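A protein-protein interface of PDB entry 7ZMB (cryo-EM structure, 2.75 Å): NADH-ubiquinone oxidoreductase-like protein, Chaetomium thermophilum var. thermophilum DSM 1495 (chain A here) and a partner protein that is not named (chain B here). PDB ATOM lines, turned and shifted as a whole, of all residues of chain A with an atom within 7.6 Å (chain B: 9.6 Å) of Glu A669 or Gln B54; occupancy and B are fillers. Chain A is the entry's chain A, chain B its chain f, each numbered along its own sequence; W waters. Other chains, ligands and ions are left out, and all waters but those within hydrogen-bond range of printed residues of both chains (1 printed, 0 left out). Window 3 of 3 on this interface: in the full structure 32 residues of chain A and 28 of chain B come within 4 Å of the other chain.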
ATOM      1  N   ARG A 396      -0.997  19.972  -9.715  1.00  0.00           N
ATOM      2  CA  ARG A 396      -2.307  20.014  -9.071  1.00  0.00           C
ATOM      3  C   ARG A 396      -3.045  18.694  -9.202  1.00  0.00           C
ATOM      4  O   ARG A 396      -3.847  18.345  -8.332  1.00  0.00           O
ATOM      5  CB  ARG A 396      -3.168  21.126  -9.657  1.00  0.00           C
ATOM      6  CG  ARG A 396      -2.717  22.527  -9.356  1.00  0.00           C
ATOM      7  CD  ARG A 396      -3.379  23.456 -10.322  1.00  0.00           C
ATOM      8  NE  ARG A 396      -4.728  23.779  -9.868  1.00  0.00           N
ATOM      9  CZ  ARG A 396      -5.793  23.861 -10.657  1.00  0.00           C
ATOM     10  NH1 ARG A 396      -5.683  23.640 -11.958  1.00  0.00           N
ATOM     11  NH2 ARG A 396      -6.972  24.156 -10.142  1.00  0.00           N
ATOM     12  N   LEU A 400      -6.170  16.471  -6.616  1.00  0.00           N
ATOM     13  CA  LEU A 400      -7.501  16.930  -6.978  1.00  0.00           C
ATOM     14  C   LEU A 400      -8.420  15.759  -7.329  1.00  0.00           C
ATOM     15  O   LEU A 400      -8.020  14.596  -7.359  1.00  0.00           O
ATOM     16  CB  LEU A 400      -7.432  17.933  -8.129  1.00  0.00           C
ATOM     17  CG  LEU A 400      -6.910  19.323  -7.772  1.00  0.00           C
ATOM     18  CD1 LEU A 400      -6.931  20.223  -8.985  1.00  0.00           C
ATOM     19  CD2 LEU A 400      -7.692  19.936  -6.624  1.00  0.00           C
ATOM     20  N   ASN A 402      -9.832  14.738 -10.334  1.00  0.00           N
ATOM     21  CA  ASN A 402      -9.369  15.200 -11.639  1.00  0.00           C
ATOM     22  C   ASN A 402     -10.424  15.006 -12.718  1.00  0.00           C
ATOM     23  O   ASN A 402     -10.698  15.922 -13.498  1.00  0.00           O
ATOM     24  CB  ASN A 402      -8.070  14.491 -12.000  1.00  0.00           C
ATOM     25  CG  ASN A 402      -6.909  15.014 -11.210  1.00  0.00           C
ATOM     26  OD1 ASN A 402      -6.579  16.188 -11.292  1.00  0.00           O
ATOM     27  ND2 ASN A 402      -6.308  14.157 -10.405  1.00  0.00           N
ATOM     28  N   LYS A 404     -14.050  15.384 -13.101  1.00  0.00           N
ATOM     29  CA  LYS A 404     -14.755  16.406 -12.347  1.00  0.00           C
ATOM     30  C   LYS A 404     -15.785  15.748 -11.438  1.00  0.00           C
ATOM     31  O   LYS A 404     -15.957  14.527 -11.473  1.00  0.00           O
ATOM     32  CB  LYS A 404     -15.418  17.374 -13.317  1.00  0.00           C
ATOM     33  CG  LYS A 404     -14.433  18.088 -14.226  1.00  0.00           C
ATOM     34  CD  LYS A 404     -13.462  18.928 -13.467  1.00  0.00           C
ATOM     35  CE  LYS A 404     -14.176  20.072 -12.815  1.00  0.00           C
ATOM     36  NZ  LYS A 404     -14.763  21.006 -13.807  1.00  0.00           N
ATOM     37  N   GLU A 609     -12.136  19.377  -6.418  1.00  0.00           N
ATOM     38  CA  GLU A 609     -11.764  19.247  -7.815  1.00  0.00           C
ATOM     39  C   GLU A 609     -10.966  20.432  -8.338  1.00  0.00           C
ATOM     40  O   GLU A 609     -10.596  20.441  -9.513  1.00  0.00           O
ATOM     41  CB  GLU A 609     -13.009  19.058  -8.668  1.00  0.00           C
ATOM     42  CG  GLU A 609     -13.799  20.312  -8.853  1.00  0.00           C
ATOM     43  CD  GLU A 609     -15.086  20.050  -9.558  1.00  0.00           C
ATOM     44  OE1 GLU A 609     -15.399  18.866  -9.778  1.00  0.00           O
ATOM     45  OE2 GLU A 609     -15.792  21.021  -9.897  1.00  0.00           O
ATOM     46  N   GLY A 610     -10.678  21.420  -7.502  1.00  0.00           N
ATOM     47  CA  GLY A 610      -9.956  22.583  -7.956  1.00  0.00           C
ATOM     48  C   GLY A 610     -10.812  23.703  -8.488  1.00  0.00           C
ATOM     49  O   GLY A 610     -10.295  24.576  -9.191  1.00  0.00           O
ATOM     50  N   ARG A 611     -12.109  23.698  -8.198  1.00  0.00           N
ATOM     51  CA  ARG A 611     -12.953  24.839  -8.506  1.00  0.00           C
ATOM     52  C   ARG A 611     -12.686  25.950  -7.506  1.00  0.00           C
ATOM     53  O   ARG A 611     -12.643  25.709  -6.299  1.00  0.00           O
ATOM     54  CB  ARG A 611     -14.428  24.444  -8.485  1.00  0.00           C
ATOM     55  CG  ARG A 611     -15.340  25.521  -9.011  1.00  0.00           C
ATOM     56  CD  ARG A 611     -16.729  24.999  -9.242  1.00  0.00           C
ATOM     57  NE  ARG A 611     -16.738  23.758 -10.004  1.00  0.00           N
ATOM     58  CZ  ARG A 611     -16.881  23.678 -11.321  1.00  0.00           C
ATOM     59  NH1 ARG A 611     -17.018  24.771 -12.047  1.00  0.00           N
ATOM     60  NH2 ARG A 611     -16.880  22.497 -11.910  1.00  0.00           N
ATOM     61  N   VAL A 612     -12.523  27.166  -8.011  1.00  0.00           N
ATOM     62  CA  VAL A 612     -12.195  28.335  -7.204  1.00  0.00           C
ATOM     63  C   VAL A 612     -13.478  29.128  -6.998  1.00  0.00           C
ATOM     64  O   VAL A 612     -14.038  29.676  -7.949  1.00  0.00           O
ATOM     65  CB  VAL A 612     -11.103  29.180  -7.876  1.00  0.00           C
ATOM     66  CG1 VAL A 612     -10.832  30.463  -7.105  1.00  0.00           C
ATOM     67  CG2 VAL A 612      -9.833  28.377  -8.013  1.00  0.00           C
ATOM     68  N   PRO A 660      -2.176  31.220 -10.734  1.00  0.00           N
ATOM     69  CA  PRO A 660      -3.072  32.158 -11.419  1.00  0.00           C
ATOM     70  C   PRO A 660      -4.500  31.668 -11.502  1.00  0.00           C
ATOM     71  O   PRO A 660      -5.399  32.470 -11.788  1.00  0.00           O
ATOM     72  CB  PRO A 660      -2.437  32.303 -12.805  1.00  0.00           C
ATOM     73  CG  PRO A 660      -1.611  31.100 -12.986  1.00  0.00           C
ATOM     74  CD  PRO A 660      -1.230  30.564 -11.654  1.00  0.00           C
ATOM     75  N   ALA A 661      -4.734  30.377 -11.252  1.00  0.00           N
ATOM     76  CA  ALA A 661      -6.089  29.850 -11.198  1.00  0.00           C
ATOM     77  C   ALA A 661      -6.912  30.521 -10.105  1.00  0.00           C
ATOM     78  O   ALA A 661      -8.139  30.608 -10.217  1.00  0.00           O
ATOM     79  CB  ALA A 661      -6.044  28.341 -10.975  1.00  0.00           C
ATOM     80  N   LEU A 662      -6.260  31.010  -9.050  1.00  0.00           N
ATOM     81  CA  LEU A 662      -6.988  31.663  -7.974  1.00  0.00           C
ATOM     82  C   LEU A 662      -7.622  32.981  -8.402  1.00  0.00           C
ATOM     83  O   LEU A 662      -8.433  33.529  -7.649  1.00  0.00           O
ATOM     84  CB  LEU A 662      -6.063  31.893  -6.783  1.00  0.00           C
ATOM     85  CG  LEU A 662      -5.731  30.696  -5.892  1.00  0.00           C
ATOM     86  CD1 LEU A 662      -4.840  31.154  -4.765  1.00  0.00           C
ATOM     87  CD2 LEU A 662      -6.967  30.031  -5.347  1.00  0.00           C
ATOM     88  N   ALA A 663      -7.272  33.508  -9.568  1.00  0.00           N
ATOM     89  CA  ALA A 663      -7.951  34.676 -10.106  1.00  0.00           C
ATOM     90  C   ALA A 663      -9.083  34.325 -11.062  1.00  0.00           C
ATOM     91  O   ALA A 663      -9.838  35.219 -11.451  1.00  0.00           O
ATOM     92  CB  ALA A 663      -6.952  35.590 -10.815  1.00  0.00           C
ATOM     93  N   ALA A 664      -9.232  33.058 -11.437  1.00  0.00           N
ATOM     94  CA  ALA A 664     -10.312  32.610 -12.314  1.00  0.00           C
ATOM     95  C   ALA A 664     -11.370  31.926 -11.459  1.00  0.00           C
ATOM     96  O   ALA A 664     -11.246  30.744 -11.127  1.00  0.00           O
ATOM     97  CB  ALA A 664      -9.787  31.673 -13.394  1.00  0.00           C
ATOM     98  N   TYR A 665     -12.422  32.657 -11.123  1.00  0.00           N
ATOM     99  CA  TYR A 665     -13.423  32.162 -10.193  1.00  0.00           C
ATOM    100  C   TYR A 665     -14.480  31.321 -10.897  1.00  0.00           C
ATOM    101  O   TYR A 665     -14.831  31.563 -12.055  1.00  0.00           O
ATOM    102  CB  TYR A 665     -14.086  33.322  -9.454  1.00  0.00           C
ATOM    103  CG  TYR A 665     -13.240  33.897  -8.341  1.00  0.00           C
ATOM    104  CD1 TYR A 665     -13.173  33.278  -7.098  1.00  0.00           C
ATOM    105  CD2 TYR A 665     -12.509  35.057  -8.532  1.00  0.00           C
ATOM    106  CE1 TYR A 665     -12.403  33.799  -6.091  1.00  0.00           C
ATOM    107  CE2 TYR A 665     -11.741  35.588  -7.529  1.00  0.00           C
ATOM    108  CZ  TYR A 665     -11.690  34.960  -6.311  1.00  0.00           C
ATOM    109  OH  TYR A 665     -10.915  35.500  -5.315  1.00  0.00           O
ATOM    110  N   VAL A 667     -14.481  28.330 -12.008  1.00  0.00           N
ATOM    111  CA  VAL A 667     -14.049  27.457 -13.086  1.00  0.00           C
ATOM    112  C   VAL A 667     -12.938  26.565 -12.559  1.00  0.00           C
ATOM    113  O   VAL A 667     -12.339  26.829 -11.516  1.00  0.00           O
ATOM    114  CB  VAL A 667     -13.576  28.251 -14.311  1.00  0.00           C
ATOM    115  CG1 VAL A 667     -14.764  28.820 -15.037  1.00  0.00           C
ATOM    116  CG2 VAL A 667     -12.669  29.364 -13.873  1.00  0.00           C
ATOM    117  N   VAL A 668     -12.684  25.485 -13.285  1.00  0.00           N
ATOM    118  CA  VAL A 668     -11.625  24.541 -12.954  1.00  0.00           C
ATOM    119  C   VAL A 668     -10.614  24.553 -14.086  1.00  0.00           C
ATOM    120  O   VAL A 668     -10.974  24.350 -15.252  1.00  0.00           O
ATOM    121  CB  VAL A 668     -12.175  23.129 -12.711  1.00  0.00           C
ATOM    122  CG1 VAL A 668     -11.085  22.227 -12.214  1.00  0.00           C
ATOM    123  CG2 VAL A 668     -13.283  23.187 -11.688  1.00  0.00           C
ATOM    124  N   GLU A 669      -9.365  24.792 -13.750  1.00  0.00           N
ATOM    125  CA  GLU A 669      -8.321  24.829 -14.761  1.00  0.00           C
ATOM    126  C   GLU A 669      -7.831  23.418 -15.073  1.00  0.00           C
ATOM    127  O   GLU A 669      -7.733  22.582 -14.176  1.00  0.00           O
ATOM    128  CB  GLU A 669      -7.154  25.694 -14.294  1.00  0.00           C
ATOM    129  CG  GLU A 669      -7.523  27.143 -14.052  1.00  0.00           C
ATOM    130  CD  GLU A 669      -7.680  27.945 -15.331  1.00  0.00           C
ATOM    131  OE1 GLU A 669      -8.104  27.379 -16.358  1.00  0.00           O
ATOM    132  OE2 GLU A 669      -7.406  29.159 -15.306  1.00  0.00           O
ATOM    133  N   PRO A 670      -7.525  23.126 -16.329  1.00  0.00           N
ATOM    134  CA  PRO A 670      -7.002  21.798 -16.667  1.00  0.00           C
ATOM    135  C   PRO A 670      -5.525  21.677 -16.330  1.00  0.00           C
ATOM    136  O   PRO A 670      -4.737  22.595 -16.557  1.00  0.00           O
ATOM    137  CB  PRO A 670      -7.239  21.703 -18.179  1.00  0.00           C
ATOM    138  CG  PRO A 670      -8.127  22.875 -18.521  1.00  0.00           C
ATOM    139  CD  PRO A 670      -7.803  23.920 -17.532  1.00  0.00           C
ATOM    140  N   VAL A 671      -5.148  20.529 -15.775  1.00  0.00           N
ATOM    141  CA  VAL A 671      -3.736  20.288 -15.498  1.00  0.00           C
ATOM    142  C   VAL A 671      -3.035  20.032 -16.828  1.00  0.00           C
ATOM    143  O   VAL A 671      -3.301  19.032 -17.498  1.00  0.00           O
ATOM    144  CB  VAL A 671      -3.531  19.123 -14.526  1.00  0.00           C
ATOM    145  CG1 VAL A 671      -2.050  18.824 -14.392  1.00  0.00           C
ATOM    146  CG2 VAL A 671      -4.141  19.447 -13.172  1.00  0.00           C
ATOM    147  N   ALA A 672      -2.181  20.968 -17.242  1.00  0.00           N
ATOM    148  CA  ALA A 672      -1.434  20.811 -18.506  1.00  0.00           C
ATOM    149  C   ALA A 672      -0.542  19.566 -18.423  1.00  0.00           C
ATOM    150  O   ALA A 672      -0.896  18.557 -19.052  1.00  0.00           O
ATOM    151  CB  ALA A 672      -0.663  22.073 -18.780  1.00  0.00           C
ATOM    152  N   LEU B  17       4.507  29.633 -13.453  1.00  0.00           N
ATOM    153  CA  LEU B  17       3.167  30.002 -13.890  1.00  0.00           C
ATOM    154  C   LEU B  17       3.149  30.002 -15.411  1.00  0.00           C
ATOM    155  O   LEU B  17       3.726  30.891 -16.040  1.00  0.00           O
ATOM    156  CB  LEU B  17       2.768  31.369 -13.340  1.00  0.00           C
ATOM    157  CG  LEU B  17       3.125  31.672 -11.887  1.00  0.00           C
ATOM    158  CD1 LEU B  17       2.811  33.111 -11.560  1.00  0.00           C
ATOM    159  CD2 LEU B  17       2.381  30.744 -10.957  1.00  0.00           C
ATOM    160  N   PHE B  18       2.492  28.990 -15.980  1.00  0.00           N
ATOM    161  CA  PHE B  18       2.417  28.859 -17.460  1.00  0.00           C
ATOM    162  C   PHE B  18       0.950  28.693 -17.841  1.00  0.00           C
ATOM    163  O   PHE B  18       0.102  28.917 -16.983  1.00  0.00           O
ATOM    164  CB  PHE B  18       3.259  27.669 -17.929  1.00  0.00           C
ATOM    165  CG  PHE B  18       2.931  26.345 -17.288  1.00  0.00           C
ATOM    166  CD1 PHE B  18       3.376  26.037 -16.012  1.00  0.00           C
ATOM    167  CD2 PHE B  18       2.188  25.393 -17.968  1.00  0.00           C
ATOM    168  CE1 PHE B  18       3.070  24.821 -15.427  1.00  0.00           C
ATOM    169  CE2 PHE B  18       1.886  24.174 -17.385  1.00  0.00           C
ATOM    170  CZ  PHE B  18       2.328  23.891 -16.115  1.00  0.00           C
ATOM    171  N   CYS B  19       0.671  28.325 -19.085  1.00  0.00           N
ATOM    172  CA  CYS B  19      -0.722  28.038 -19.503  1.00  0.00           C
ATOM    173  C   CYS B  19      -0.743  26.746 -20.308  1.00  0.00           C
ATOM    174  O   CYS B  19       0.314  26.372 -20.836  1.00  0.00           O
ATOM    175  CB  CYS B  19      -1.327  29.147 -20.355  1.00  0.00           C
ATOM    176  SG  CYS B  19      -0.439  29.465 -21.904  1.00  0.00           S
ATOM    177  N   GLN B  20      -1.890  26.077 -20.348  1.00  0.00           N
ATOM    178  CA  GLN B  20      -2.084  24.854 -21.162  1.00  0.00           C
ATOM    179  C   GLN B  20      -2.020  25.196 -22.648  1.00  0.00           C
ATOM    180  O   GLN B  20      -1.567  24.334 -23.418  1.00  0.00           O
ATOM    181  CB  GLN B  20      -3.488  24.324 -20.875  1.00  0.00           C
ATOM    182  CG  GLN B  20      -3.809  24.139 -19.395  1.00  0.00           C
ATOM    183  CD  GLN B  20      -4.314  25.374 -18.687  1.00  0.00           C
ATOM    184  OE1 GLN B  20      -4.358  26.469 -19.243  1.00  0.00           O
ATOM    185  NE2 GLN B  20      -4.700  25.206 -17.433  1.00  0.00           N
ATOM    186  N   THR B  21      -2.493  26.379 -23.046  1.00  0.00           N
ATOM    187  CA  THR B  21      -2.624  26.767 -24.478  1.00  0.00           C
ATOM    188  C   THR B  21      -1.313  27.097 -25.195  1.00  0.00           C
ATOM    189  O   THR B  21      -0.293  27.260 -24.515  1.00  0.00           O
ATOM    190  CB  THR B  21      -3.524  27.997 -24.607  1.00  0.00           C
ATOM    191  OG1 THR B  21      -2.888  29.090 -23.945  1.00  0.00           O
ATOM    192  CG2 THR B  21      -4.902  27.778 -24.023  1.00  0.00           C
ATOM    193  N   SER B  22      -1.356  27.152 -26.535  1.00  0.00           N
ATOM    194  CA  SER B  22      -0.168  27.541 -27.345  1.00  0.00           C
ATOM    195  C   SER B  22      -0.130  29.062 -27.536  1.00  0.00           C
ATOM    196  O   SER B  22       0.779  29.528 -28.246  1.00  0.00           O
ATOM    197  CB  SER B  22      -0.170  26.827 -28.669  1.00  0.00           C
ATOM    198  OG  SER B  22      -1.293  27.216 -29.446  1.00  0.00           O
ATOM    199  N   GLN B  23      -1.082  29.802 -26.957  1.00  0.00           N
ATOM    200  CA  GLN B  23      -1.039  31.260 -26.986  1.00  0.00           C
ATOM    201  C   GLN B  23       0.357  31.760 -26.661  1.00  0.00           C
ATOM    202  O   GLN B  23       0.866  32.689 -27.299  1.00  0.00           O
ATOM    203  CB  GLN B  23      -2.047  31.839 -25.996  1.00  0.00           C
ATOM    204  CG  GLN B  23      -1.779  33.286 -25.637  1.00  0.00           C
ATOM    205  CD  GLN B  23      -2.462  33.700 -24.360  1.00  0.00           C
ATOM    206  OE1 GLN B  23      -3.195  32.921 -23.762  1.00  0.00           O
ATOM    207  NE2 GLN B  23      -2.235  34.936 -23.941  1.00  0.00           N
ATOM    208  N   HIS B  24       0.992  31.112 -25.677  1.00  0.00           N
ATOM    209  CA  HIS B  24       2.421  31.407 -25.433  1.00  0.00           C
ATOM    210  C   HIS B  24       3.165  30.158 -25.905  1.00  0.00           C
ATOM    211  O   HIS B  24       2.538  29.083 -25.836  1.00  0.00           O
ATOM    212  CB  HIS B  24       2.660  31.704 -23.953  1.00  0.00           C
ATOM    213  CG  HIS B  24       1.776  32.771 -23.400  1.00  0.00           C
ATOM    214  ND1 HIS B  24       0.683  32.485 -22.610  1.00  0.00           N
ATOM    215  CD2 HIS B  24       1.822  34.115 -23.513  1.00  0.00           C
ATOM    216  CE1 HIS B  24       0.094  33.608 -22.258  1.00  0.00           C
ATOM    217  NE2 HIS B  24       0.771  34.622 -22.801  1.00  0.00           N
ATOM    218  N   ARG B  29       6.360  24.550 -21.187  1.00  0.00           N
ATOM    219  CA  ARG B  29       5.824  23.182 -20.974  1.00  0.00           C
ATOM    220  C   ARG B  29       6.857  22.164 -21.446  1.00  0.00           C
ATOM    221  O   ARG B  29       6.972  21.126 -20.793  1.00  0.00           O
ATOM    222  CB  ARG B  29       4.478  23.000 -21.673  1.00  0.00           C
ATOM    223  CG  ARG B  29       3.322  22.686 -20.734  1.00  0.00           C
ATOM    224  CD  ARG B  29       1.973  22.729 -21.427  1.00  0.00           C
ATOM    225  NE  ARG B  29       1.695  24.052 -21.964  1.00  0.00           N
ATOM    226  CZ  ARG B  29       1.787  24.386 -23.245  1.00  0.00           C
ATOM    227  NH1 ARG B  29       1.528  25.625 -23.621  1.00  0.00           N
ATOM    228  NH2 ARG B  29       2.129  23.485 -24.149  1.00  0.00           N
ATOM    229  N   LEU B  50       4.077  23.731  -9.941  1.00  0.00           N
ATOM    230  CA  LEU B  50       3.671  23.952 -11.322  1.00  0.00           C
ATOM    231  C   LEU B  50       2.217  24.395 -11.333  1.00  0.00           C
ATOM    232  O   LEU B  50       1.314  23.595 -11.068  1.00  0.00           O
ATOM    233  CB  LEU B  50       3.868  22.686 -12.145  1.00  0.00           C
ATOM    234  CG  LEU B  50       5.305  22.175 -12.113  1.00  0.00           C
ATOM    235  CD1 LEU B  50       5.402  20.769 -12.644  1.00  0.00           C
ATOM    236  CD2 LEU B  50       6.171  23.107 -12.909  1.00  0.00           C
ATOM    237  N   ARG B  51       1.987  25.667 -11.631  1.00  0.00           N
ATOM    238  CA  ARG B  51       0.653  26.249 -11.608  1.00  0.00           C
ATOM    239  C   ARG B  51       0.347  26.850 -12.966  1.00  0.00           C
ATOM    240  O   ARG B  51       1.157  27.602 -13.511  1.00  0.00           O
ATOM    241  CB  ARG B  51       0.540  27.311 -10.515  1.00  0.00           C
ATOM    242  CG  ARG B  51       0.881  26.772  -9.151  1.00  0.00           C
ATOM    243  CD  ARG B  51      -0.171  25.786  -8.718  1.00  0.00           C
ATOM    244  NE  ARG B  51       0.067  25.266  -7.380  1.00  0.00           N
ATOM    245  CZ  ARG B  51       0.525  24.046  -7.138  1.00  0.00           C
ATOM    246  NH1 ARG B  51       0.712  23.644  -5.891  1.00  0.00           N
ATOM    247  NH2 ARG B  51       0.796  23.233  -8.148  1.00  0.00           N
ATOM    248  N   GLU B  52      -0.809  26.521 -13.514  1.00  0.00           N
ATOM    249  CA  GLU B  52      -1.163  26.974 -14.843  1.00  0.00           C
ATOM    250  C   GLU B  52      -2.592  27.488 -14.861  1.00  0.00           C
ATOM    251  O   GLU B  52      -3.432  27.083 -14.056  1.00  0.00           O
ATOM    252  CB  GLU B  52      -0.971  25.862 -15.888  1.00  0.00           C
ATOM    253  CG  GLU B  52      -1.854  24.661 -15.711  1.00  0.00           C
ATOM    254  CD  GLU B  52      -1.197  23.569 -14.901  1.00  0.00           C
ATOM    255  OE1 GLU B  52      -0.369  23.881 -14.021  1.00  0.00           O
ATOM    256  OE2 GLU B  52      -1.490  22.388 -15.156  1.00  0.00           O
ATOM    257  N   ALA B  53      -2.848  28.403 -15.787  1.00  0.00           N
ATOM    258  CA  ALA B  53      -4.152  29.026 -15.939  1.00  0.00           C
ATOM    259  C   ALA B  53      -4.194  29.664 -17.312  1.00  0.00           C
ATOM    260  O   ALA B  53      -3.177  30.154 -17.808  1.00  0.00           O
ATOM    261  CB  ALA B  53      -4.419  30.066 -14.849  1.00  0.00           C
ATOM    262  N   GLN B  54      -5.378  29.647 -17.920  1.00  0.00           N
ATOM    263  CA  GLN B  54      -5.529  30.135 -19.280  1.00  0.00           C
ATOM    264  C   GLN B  54      -5.020  31.562 -19.402  1.00  0.00           C
ATOM    265  O   GLN B  54      -5.341  32.424 -18.579  1.00  0.00           O
ATOM    266  CB  GLN B  54      -6.992  30.065 -19.703  1.00  0.00           C
ATOM    267  CG  GLN B  54      -7.708  28.797 -19.281  1.00  0.00           C
ATOM    268  CD  GLN B  54      -7.668  27.728 -20.355  1.00  0.00           C
ATOM    269  OE1 GLN B  54      -8.058  27.965 -21.497  1.00  0.00           O
ATOM    270  NE2 GLN B  54      -7.193  26.544 -19.993  1.00  0.00           N
ATOM    271  N   GLY B  55      -4.222  31.803 -20.435  1.00  0.00           N
ATOM    272  CA  GLY B  55      -3.687  33.124 -20.667  1.00  0.00           C
ATOM    273  C   GLY B  55      -2.724  33.605 -19.614  1.00  0.00           C
ATOM    274  O   GLY B  55      -2.754  34.780 -19.248  1.00  0.00           O
ATOM    275  N   THR B  56      -1.866  32.731 -19.116  1.00  0.00           N
ATOM    276  CA  THR B  56      -0.867  33.120 -18.138  1.00  0.00           C
ATOM    277  C   THR B  56       0.460  33.283 -18.861  1.00  0.00           C
ATOM    278  O   THR B  56       0.944  32.344 -19.498  1.00  0.00           O
ATOM    279  CB  THR B  56      -0.753  32.082 -17.026  1.00  0.00           C
ATOM    280  OG1 THR B  56      -2.018  31.954 -16.377  1.00  0.00           O
ATOM    281  CG2 THR B  56       0.255  32.526 -15.999  1.00  0.00           C
ATOM    282  N   ILE B  57       1.039  34.474 -18.771  1.00  0.00           N
ATOM    283  CA  ILE B  57       2.373  34.659 -19.344  1.00  0.00           C
ATOM    284  C   ILE B  57       3.367  33.788 -18.584  1.00  0.00           C
ATOM    285  O   ILE B  57       3.415  33.846 -17.341  1.00  0.00           O
ATOM    286  CB  ILE B  57       2.775  36.141 -19.290  1.00  0.00           C
ATOM    287  CG1 ILE B  57       1.866  36.956 -20.203  1.00  0.00           C
ATOM    288  CG2 ILE B  57       4.217  36.301 -19.685  1.00  0.00           C
ATOM    289  CD1 ILE B  57       1.949  38.435 -19.998  1.00  0.00           C
ATOM    290  N   PRO B  58       4.159  32.962 -19.265  1.00  0.00           N
ATOM    291  CA  PRO B  58       5.118  32.108 -18.563  1.00  0.00           C
ATOM    292  C   PRO B  58       6.102  32.914 -17.732  1.00  0.00           C
ATOM    293  O   PRO B  58       6.502  34.020 -18.099  1.00  0.00           O
ATOM    294  CB  PRO B  58       5.810  31.354 -19.700  1.00  0.00           C
ATOM    295  CG  PRO B  58       4.768  31.258 -20.731  1.00  0.00           C
ATOM    296  CD  PRO B  58       4.017  32.561 -20.671  1.00  0.00           C
HETATM  297  O   HOH W   1      -3.066  26.548 -11.127  1.00  0.00           O
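The backbone NH (N) of Ala A672 is in hydrogen-bond range of the side-chain carboxylate (OE2) of Glu B52.
The backbone carbonyl oxygen (O) of Pro A670 lies within hydrogen-bond range of the side-chain amide nitrogen (NE2) of Gln B20 (2.8 Å).
The side-chain carboxylate (OE2) of Glu A669 lies within hydrogen-bond range of the backbone NH (N) of Gln B54, 3.3 Å away.
The backbone NH (N) of Ala B53 is in hydrogen-bond range of the backbone carbonyl oxygen (O) of Phe B18 (3.2 Å).
A ring nitrogen (ND1) of His B24 is in hydrogen-bond range of the backbone carbonyl oxygen (O) of Thr B56 (3.1 Å).
The backbone carbonyl oxygen (O) of Arg B51 lies within hydrogen-bond range of the backbone NH (N) of Phe B18 (3.1 Å).
The backbone carbonyl oxygen (O) of Glu A669 lies within hydrogen-bond range of the guanidinium group (NH1) of Arg A396, at 3.2 Å.
O of Cys B19 is in hydrogen-bond range of NE of Arg B29 (2.9 Å).
The guanidinium group (NH1) of Arg B29 lies within hydrogen-bond range of the backbone carbonyl oxygen (O) of Thr B21, at 2.6 Å.
Among the printed residues, pairs that only touch across the chains: Arg A396 with Arg B51, Pro A660 with Leu B17, Pro A660 with Arg B51, Pro A660 with Ala B53, Pro A660 with Thr B56, Ala A661 with Ala B53, Glu A669 with Glu B52, Glu A669 with Ala B53, Pro A670 with Glu B52, Pro A670 with Gln B54, Val A671 with Glu B52, Ala A672 with Phe B18, Ala A672 with Gln B20 and Ala A672 with Arg B29.
Of the printed residues of chain B, Pro A660 touches Leu B17 (3.7 Å), Arg B51 (3.9 Å), Ala B53 (3.5 Å) and Thr B56 (3.5 Å).
Ala A661 touches just one residue of chain B: Ala B53 (3.6 Å).
No residue of chain B comes within 4 Å of Val A668.
Of the printed residues of chain B, Glu A669 touches Glu B52, Ala B53 and Gln B54.
Of chain B, only Gln B20, Glu B52 and Gln B54 come within 4 Å of Pro A670.
Of the printed residues of chain A, Phe B18 touches Ala A672 (3.6 Å).
Of the printed residues of chain A, Gln B20 touches Pro A670 and Ala A672.
Of the printed residues of chain A, Arg B51 touches Arg A396 (3.8 Å) and Pro A660 (3.9 Å).
Of chain A, only Pro A660, Ala A661 and Glu A669 come within 4 Å of Ala B53.
Printed residues of chain A within 4 Å of Gln B54: Glu A669 (3.3 Å) and Pro A670 (3.6 Å).
The nearest printed residue of chain B that does not touch Glu A669 is Gln B20 (4.01 Å).
Of the 20 printed residues of chain A, 7 touch a printed residue of chain B.
Water W1 bridges O of Glu B52 and NE of Arg A396.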
